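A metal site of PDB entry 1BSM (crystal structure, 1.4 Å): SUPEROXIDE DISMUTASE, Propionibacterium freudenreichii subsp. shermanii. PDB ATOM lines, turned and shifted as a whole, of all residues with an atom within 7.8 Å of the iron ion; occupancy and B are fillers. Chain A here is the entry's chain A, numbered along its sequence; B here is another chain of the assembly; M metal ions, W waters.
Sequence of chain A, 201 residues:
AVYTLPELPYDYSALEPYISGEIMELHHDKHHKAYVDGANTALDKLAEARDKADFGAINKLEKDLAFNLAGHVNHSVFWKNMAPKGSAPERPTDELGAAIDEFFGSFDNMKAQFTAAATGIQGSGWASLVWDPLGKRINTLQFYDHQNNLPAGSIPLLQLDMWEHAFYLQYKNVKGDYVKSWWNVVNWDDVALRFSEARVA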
ATOM      1  N   HIS A  27       6.342  32.109 -33.181  1.00  0.00           N
ATOM      2  CA  HIS A  27       6.569  31.285 -32.003  1.00  0.00           C
ATOM      3  C   HIS A  27       7.678  30.256 -32.193  1.00  0.00           C
ATOM      4  O   HIS A  27       8.527  30.074 -31.312  1.00  0.00           O
ATOM      5  CB  HIS A  27       5.256  30.582 -31.647  1.00  0.00           C
ATOM      6  CG  HIS A  27       5.160  30.158 -30.215  1.00  0.00           C
ATOM      7  ND1 HIS A  27       4.079  29.463 -29.720  1.00  0.00           N
ATOM      8  CD2 HIS A  27       6.012  30.328 -29.174  1.00  0.00           C
ATOM      9  CE1 HIS A  27       4.262  29.238 -28.435  1.00  0.00           C
ATOM     10  NE2 HIS A  27       5.417  29.751 -28.076  1.00  0.00           N
ATOM     11  N   HIS A  28       7.683  29.603 -33.343  1.00  0.00           N
ATOM     12  CA  HIS A  28       8.683  28.586 -33.654  1.00  0.00           C
ATOM     13  C   HIS A  28      10.007  29.167 -34.138  1.00  0.00           C
ATOM     14  O   HIS A  28      11.052  28.978 -33.511  1.00  0.00           O
ATOM     15  CB  HIS A  28       8.126  27.600 -34.694  1.00  0.00           C
ATOM     16  CG  HIS A  28       9.114  26.567 -35.128  1.00  0.00           C
ATOM     17  ND1 HIS A  28       9.325  25.393 -34.435  1.00  0.00           N
ATOM     18  CD2 HIS A  28       9.970  26.535 -36.188  1.00  0.00           C
ATOM     19  CE1 HIS A  28      10.261  24.680 -35.050  1.00  0.00           C
ATOM     20  NE2 HIS A  28      10.663  25.353 -36.106  1.00  0.00           N
ATOM     21  N   HIS A  31      10.843  32.671 -31.224  1.00  0.00           N
ATOM     22  CA  HIS A  31      10.877  32.328 -29.806  1.00  0.00           C
ATOM     23  C   HIS A  31      11.628  31.054 -29.421  1.00  0.00           C
ATOM     24  O   HIS A  31      12.540  31.108 -28.598  1.00  0.00           O
ATOM     25  CB  HIS A  31       9.459  32.319 -29.222  1.00  0.00           C
ATOM     26  CG  HIS A  31       8.899  33.691 -29.033  1.00  0.00           C
ATOM     27  ND1 HIS A  31       8.148  34.338 -29.997  1.00  0.00           N
ATOM     28  CD2 HIS A  31       9.006  34.556 -27.999  1.00  0.00           C
ATOM     29  CE1 HIS A  31       7.818  35.539 -29.564  1.00  0.00           C
ATOM     30  NE2 HIS A  31       8.332  35.695 -28.356  1.00  0.00           N
ATOM     31  N   HIS A  32      11.262  29.933 -30.020  1.00  0.00           N
ATOM     32  CA  HIS A  32      11.928  28.663 -29.705  1.00  0.00           C
ATOM     33  C   HIS A  32      13.409  28.715 -30.059  1.00  0.00           C
ATOM     34  O   HIS A  32      14.257  28.251 -29.289  1.00  0.00           O
ATOM     35  CB  HIS A  32      11.235  27.501 -30.423  1.00  0.00           C
ATOM     36  CG  HIS A  32      11.565  26.156 -29.835  1.00  0.00           C
ATOM     37  ND1 HIS A  32      10.903  25.004 -30.204  1.00  0.00           N
ATOM     38  CD2 HIS A  32      12.470  25.780 -28.903  1.00  0.00           C
ATOM     39  CE1 HIS A  32      11.391  23.977 -29.532  1.00  0.00           C
ATOM     40  NE2 HIS A  32      12.343  24.430 -28.730  1.00  0.00           N
ATOM     41  N   TYR A  35      15.542  30.231 -27.356  1.00  0.00           N
ATOM     42  CA  TYR A  35      15.782  29.363 -26.199  1.00  0.00           C
ATOM     43  C   TYR A  35      16.905  28.381 -26.490  1.00  0.00           C
ATOM     44  O   TYR A  35      17.738  28.111 -25.616  1.00  0.00           O
ATOM     45  CB  TYR A  35      14.517  28.581 -25.824  1.00  0.00           C
ATOM     46  CG  TYR A  35      13.355  29.457 -25.448  1.00  0.00           C
ATOM     47  CD1 TYR A  35      13.507  30.532 -24.563  1.00  0.00           C
ATOM     48  CD2 TYR A  35      12.095  29.245 -25.998  1.00  0.00           C
ATOM     49  CE1 TYR A  35      12.450  31.371 -24.249  1.00  0.00           C
ATOM     50  CE2 TYR A  35      11.025  30.071 -25.696  1.00  0.00           C
ATOM     51  CZ  TYR A  35      11.209  31.130 -24.820  1.00  0.00           C
ATOM     52  OH  TYR A  35      10.149  31.958 -24.522  1.00  0.00           O
ATOM     53  N   GLY A  71      12.614  26.413 -21.588  1.00  0.00           N
ATOM     54  CA  GLY A  71      11.849  26.929 -22.717  1.00  0.00           C
ATOM     55  C   GLY A  71      11.961  25.973 -23.889  1.00  0.00           C
ATOM     56  O   GLY A  71      10.993  25.726 -24.609  1.00  0.00           O
ATOM     57  N   ASN A  74       9.901  22.746 -22.857  1.00  0.00           N
ATOM     58  CA  ASN A  74       8.479  23.047 -22.909  1.00  0.00           C
ATOM     59  C   ASN A  74       7.911  23.187 -24.316  1.00  0.00           C
ATOM     60  O   ASN A  74       6.846  22.643 -24.611  1.00  0.00           O
ATOM     61  CB  ASN A  74       8.173  24.318 -22.106  1.00  0.00           C
ATOM     62  CG  ASN A  74       8.385  24.145 -20.614  1.00  0.00           C
ATOM     63  OD1 ASN A  74       8.490  23.025 -20.122  1.00  0.00           O
ATOM     64  ND2 ASN A  74       8.442  25.257 -19.884  1.00  0.00           N
ATOM     65  N   HIS A  75       8.621  23.904 -25.190  1.00  0.00           N
ATOM     66  CA  HIS A  75       8.161  24.086 -26.553  1.00  0.00           C
ATOM     67  C   HIS A  75       8.299  22.844 -27.425  1.00  0.00           C
ATOM     68  O   HIS A  75       7.474  22.610 -28.301  1.00  0.00           O
ATOM     69  CB  HIS A  75       8.845  25.290 -27.207  1.00  0.00           C
ATOM     70  CG  HIS A  75       8.387  26.596 -26.644  1.00  0.00           C
ATOM     71  ND1 HIS A  75       8.889  27.118 -25.470  1.00  0.00           N
ATOM     72  CD2 HIS A  75       7.447  27.473 -27.074  1.00  0.00           C
ATOM     73  CE1 HIS A  75       8.273  28.257 -25.201  1.00  0.00           C
ATOM     74  NE2 HIS A  75       7.391  28.489 -26.161  1.00  0.00           N
ATOM     75  N   PHE A  78       5.405  20.943 -26.519  1.00  0.00           N
ATOM     76  CA  PHE A  78       4.249  21.712 -26.997  1.00  0.00           C
ATOM     77  C   PHE A  78       3.892  21.426 -28.463  1.00  0.00           C
ATOM     78  O   PHE A  78       2.721  21.163 -28.771  1.00  0.00           O
ATOM     79  CB  PHE A  78       4.515  23.214 -26.798  1.00  0.00           C
ATOM     80  CG  PHE A  78       3.333  24.096 -27.087  1.00  0.00           C
ATOM     81  CD1 PHE A  78       2.125  23.913 -26.415  1.00  0.00           C
ATOM     82  CD2 PHE A  78       3.438  25.120 -28.012  1.00  0.00           C
ATOM     83  CE1 PHE A  78       1.041  24.746 -26.655  1.00  0.00           C
ATOM     84  CE2 PHE A  78       2.360  25.964 -28.260  1.00  0.00           C
ATOM     85  CZ  PHE A  78       1.155  25.773 -27.583  1.00  0.00           C
ATOM     86  N   TRP A  79       4.892  21.437 -29.337  1.00  0.00           N
ATOM     87  CA  TRP A  79       4.661  21.197 -30.766  1.00  0.00           C
ATOM     88  C   TRP A  79       4.086  19.807 -31.033  1.00  0.00           C
ATOM     89  O   TRP A  79       3.075  19.674 -31.738  1.00  0.00           O
ATOM     90  CB  TRP A  79       5.925  21.388 -31.594  1.00  0.00           C
ATOM     91  CG  TRP A  79       6.685  22.669 -31.343  1.00  0.00           C
ATOM     92  CD1 TRP A  79       8.038  22.801 -31.209  1.00  0.00           C
ATOM     93  CD2 TRP A  79       6.155  24.006 -31.236  1.00  0.00           C
ATOM     94  NE1 TRP A  79       8.380  24.122 -31.036  1.00  0.00           N
ATOM     95  CE2 TRP A  79       7.252  24.881 -31.049  1.00  0.00           C
ATOM     96  CE3 TRP A  79       4.859  24.554 -31.295  1.00  0.00           C
ATOM     97  CZ2 TRP A  79       7.089  26.263 -30.912  1.00  0.00           C
ATOM     98  CZ3 TRP A  79       4.702  25.915 -31.157  1.00  0.00           C
ATOM     99  CH2 TRP A  79       5.812  26.764 -30.979  1.00  0.00           C
ATOM    100  N   GLY A 125       3.455  31.721 -18.019  1.00  0.00           N
ATOM    101  CA  GLY A 125       3.494  30.372 -17.498  1.00  0.00           C
ATOM    102  C   GLY A 125       2.926  29.300 -18.398  1.00  0.00           C
ATOM    103  O   GLY A 125       2.674  29.527 -19.580  1.00  0.00           O
ATOM    104  N   TRP A 126       2.730  28.115 -17.812  1.00  0.00           N
ATOM    105  CA  TRP A 126       2.200  26.957 -18.509  1.00  0.00           C
ATOM    106  C   TRP A 126       1.279  26.152 -17.609  1.00  0.00           C
ATOM    107  O   TRP A 126       1.393  26.197 -16.389  1.00  0.00           O
ATOM    108  CB  TRP A 126       3.326  25.995 -18.915  1.00  0.00           C
ATOM    109  CG  TRP A 126       4.363  26.532 -19.825  1.00  0.00           C
ATOM    110  CD1 TRP A 126       5.302  27.475 -19.524  1.00  0.00           C
ATOM    111  CD2 TRP A 126       4.577  26.171 -21.185  1.00  0.00           C
ATOM    112  NE1 TRP A 126       6.078  27.725 -20.617  1.00  0.00           N
ATOM    113  CE2 TRP A 126       5.662  26.935 -21.655  1.00  0.00           C
ATOM    114  CE3 TRP A 126       3.960  25.255 -22.060  1.00  0.00           C
ATOM    115  CZ2 TRP A 126       6.144  26.835 -22.966  1.00  0.00           C
ATOM    116  CZ3 TRP A 126       4.441  25.155 -23.371  1.00  0.00           C
ATOM    117  CH2 TRP A 126       5.526  25.939 -23.805  1.00  0.00           C
ATOM    118  N   HIS A 146       9.085  29.428 -17.429  1.00  0.00           N
ATOM    119  CA  HIS A 146       9.329  28.121 -18.053  1.00  0.00           C
ATOM    120  C   HIS A 146       9.880  27.140 -17.040  1.00  0.00           C
ATOM    121  O   HIS A 146       9.561  25.946 -17.084  1.00  0.00           O
ATOM    122  CB  HIS A 146      10.376  28.230 -19.159  1.00  0.00           C
ATOM    123  CG  HIS A 146       9.921  28.971 -20.374  1.00  0.00           C
ATOM    124  ND1 HIS A 146      10.673  29.957 -20.962  1.00  0.00           N
ATOM    125  CD2 HIS A 146       8.800  28.862 -21.119  1.00  0.00           C
ATOM    126  CE1 HIS A 146      10.038  30.429 -22.016  1.00  0.00           C
ATOM    127  NE2 HIS A 146       8.894  29.774 -22.137  1.00  0.00           N
ATOM    128  N   ASP A 161       1.119  26.405 -23.588  1.00  0.00           N
ATOM    129  CA  ASP A 161       1.865  27.651 -23.445  1.00  0.00           C
ATOM    130  C   ASP A 161       0.908  28.799 -23.139  1.00  0.00           C
ATOM    131  O   ASP A 161       0.071  29.155 -23.972  1.00  0.00           O
ATOM    132  CB  ASP A 161       2.653  27.946 -24.724  1.00  0.00           C
ATOM    133  CG  ASP A 161       3.690  29.050 -24.549  1.00  0.00           C
ATOM    134  OD1 ASP A 161       3.737  29.684 -23.473  1.00  0.00           O
ATOM    135  OD2 ASP A 161       4.480  29.273 -25.489  1.00  0.00           O
ATOM    136  N   MET A 162       1.023  29.363 -21.940  1.00  0.00           N
ATOM    137  CA  MET A 162       0.165  30.469 -21.552  1.00  0.00           C
ATOM    138  C   MET A 162       0.882  31.812 -21.560  1.00  0.00           C
ATOM    139  O   MET A 162       0.426  32.784 -20.945  1.00  0.00           O
ATOM    140  CB  MET A 162      -0.510  30.195 -20.202  1.00  0.00           C
ATOM    141  CG  MET A 162      -1.559  29.088 -20.247  1.00  0.00           C
ATOM    142  SD  MET A 162      -2.820  29.315 -21.538  1.00  0.00           S
ATOM    143  CE  MET A 162      -3.677  30.776 -20.941  1.00  0.00           C
ATOM    144  N   TRP A 163       2.033  31.869 -22.228  1.00  0.00           N
ATOM    145  CA  TRP A 163       2.761  33.127 -22.366  1.00  0.00           C
ATOM    146  C   TRP A 163       1.898  33.919 -23.356  1.00  0.00           C
ATOM    147  O   TRP A 163       1.333  33.333 -24.292  1.00  0.00           O
ATOM    148  CB  TRP A 163       4.149  32.909 -22.967  1.00  0.00           C
ATOM    149  CG  TRP A 163       5.192  32.504 -21.985  1.00  0.00           C
ATOM    150  CD1 TRP A 163       5.164  31.429 -21.142  1.00  0.00           C
ATOM    151  CD2 TRP A 163       6.456  33.147 -21.770  1.00  0.00           C
ATOM    152  NE1 TRP A 163       6.328  31.367 -20.422  1.00  0.00           N
ATOM    153  CE2 TRP A 163       7.138  32.404 -20.784  1.00  0.00           C
ATOM    154  CE3 TRP A 163       7.077  34.281 -22.321  1.00  0.00           C
ATOM    155  CZ2 TRP A 163       8.423  32.753 -20.339  1.00  0.00           C
ATOM    156  CZ3 TRP A 163       8.352  34.629 -21.872  1.00  0.00           C
ATOM    157  CH2 TRP A 163       9.004  33.867 -20.891  1.00  0.00           C
ATOM    158  N   GLU A 164       1.812  35.224 -23.157  1.00  0.00           N
ATOM    159  CA  GLU A 164       0.995  36.069 -24.034  1.00  0.00           C
ATOM    160  C   GLU A 164       1.344  35.985 -25.525  1.00  0.00           C
ATOM    161  O   GLU A 164       0.449  36.107 -26.364  1.00  0.00           O
ATOM    162  CB  GLU A 164       1.005  37.506 -23.526  1.00  0.00           C
ATOM    163  CG  GLU A 164       0.391  37.624 -22.121  1.00  0.00           C
ATOM    164  CD  GLU A 164       0.415  39.030 -21.570  1.00  0.00           C
ATOM    165  OE1 GLU A 164       1.433  39.721 -21.708  1.00  0.00           O
ATOM    166  OE2 GLU A 164      -0.609  39.439 -20.967  1.00  0.00           O
ATOM    167  N   HIS A 165       2.601  35.714 -25.857  1.00  0.00           N
ATOM    168  CA  HIS A 165       3.002  35.609 -27.258  1.00  0.00           C
ATOM    169  C   HIS A 165       2.374  34.419 -27.970  1.00  0.00           C
ATOM    170  O   HIS A 165       2.356  34.362 -29.205  1.00  0.00           O
ATOM    171  CB  HIS A 165       4.534  35.538 -27.397  1.00  0.00           C
ATOM    172  CG  HIS A 165       5.144  34.295 -26.825  1.00  0.00           C
ATOM    173  ND1 HIS A 165       6.019  34.329 -25.754  1.00  0.00           N
ATOM    174  CD2 HIS A 165       5.027  32.994 -27.166  1.00  0.00           C
ATOM    175  CE1 HIS A 165       6.417  33.096 -25.476  1.00  0.00           C
ATOM    176  NE2 HIS A 165       5.836  32.265 -26.321  1.00  0.00           N
ATOM    177  N   ALA A 166       1.859  33.459 -27.194  1.00  0.00           N
ATOM    178  CA  ALA A 166       1.241  32.269 -27.746  1.00  0.00           C
ATOM    179  C   ALA A 166      -0.212  32.452 -28.158  1.00  0.00           C
ATOM    180  O   ALA A 166      -0.757  31.604 -28.873  1.00  0.00           O
ATOM    181  CB  ALA A 166       1.359  31.114 -26.756  1.00  0.00           C
ATOM    182  N   TYR A 178      -8.755  30.969 -25.963  1.00  0.00           N
ATOM    183  CA  TYR A 178      -7.529  30.340 -26.444  1.00  0.00           C
ATOM    184  C   TYR A 178      -7.459  28.900 -25.952  1.00  0.00           C
ATOM    185  O   TYR A 178      -7.188  27.987 -26.741  1.00  0.00           O
ATOM    186  CB  TYR A 178      -6.316  31.128 -25.971  1.00  0.00           C
ATOM    187  CG  TYR A 178      -4.980  30.422 -26.122  1.00  0.00           C
ATOM    188  CD1 TYR A 178      -4.543  29.939 -27.360  1.00  0.00           C
ATOM    189  CD2 TYR A 178      -4.139  30.263 -25.029  1.00  0.00           C
ATOM    190  CE1 TYR A 178      -3.294  29.336 -27.501  1.00  0.00           C
ATOM    191  CE2 TYR A 178      -2.886  29.671 -25.154  1.00  0.00           C
ATOM    192  CZ  TYR A 178      -2.473  29.206 -26.386  1.00  0.00           C
ATOM    193  OH  TYR A 178      -1.219  28.652 -26.514  1.00  0.00           O
ATOM    194  N   GLU B 164       4.371  41.135 -22.575  1.00  0.00           N
ATOM    195  CA  GLU B 164       4.091  41.012 -24.000  1.00  0.00           C
ATOM    196  C   GLU B 164       2.814  41.696 -24.500  1.00  0.00           C
ATOM    197  O   GLU B 164       2.780  42.162 -25.631  1.00  0.00           O
ATOM    198  CB  GLU B 164       4.137  39.541 -24.421  1.00  0.00           C
ATOM    199  CG  GLU B 164       5.508  38.901 -24.177  1.00  0.00           C
ATOM    200  CD  GLU B 164       5.562  37.441 -24.545  1.00  0.00           C
ATOM    201  OE1 GLU B 164       4.637  36.691 -24.160  1.00  0.00           O
ATOM    202  OE2 GLU B 164       6.534  37.028 -25.195  1.00  0.00           O
HETATM  203 FE    FE M   1       6.091  30.180 -25.999  1.00  0.00          FE
HETATM  204  O   HOH W   1       6.484  30.399 -23.917  1.00  0.00           O
HETATM  205  O   HOH W   2       8.229  31.026 -26.554  1.00  0.00           O
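Water W1 bridges OD1 of Asp 161 and NE2 of His 146.
The iron ion is bound by OD2 of Asp 161 (1.9 Å), NE2 of His 165 (2.1 Å), water W1 (2.1 Å), NE2 of His 75 (2.1 Å), NE2 of His 27 (2.2 Å) and water W2 (2.4 Å).
Within 4 Å of the iron ion: His 27, His 75, Asp 161 and His 165.
The nearest printed residue that does not touch the iron ion is Trp 126 (4.5 Å).
The backbone carbonyl oxygen of His 27 lies within hydrogen-bond range of the backbone NH of His 32 (3.0 Å).
N of Trp 163 is in hydrogen-bond range of OD1 of Asp 161.
ND1 of His 75 lies within hydrogen-bond range of O of Gly 71 (2.7 Å).
O of His 75 sits close to NE1 of Trp 79 (3.3 Å).
A ring nitrogen (ND1) of His 165 is in hydrogen-bond range of the side-chain carboxylate of Glu 164 of chain B, at 2.8 Å.
O of Asp 161 lies within hydrogen-bond range of OH of Tyr 178, 2.9 Å away.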
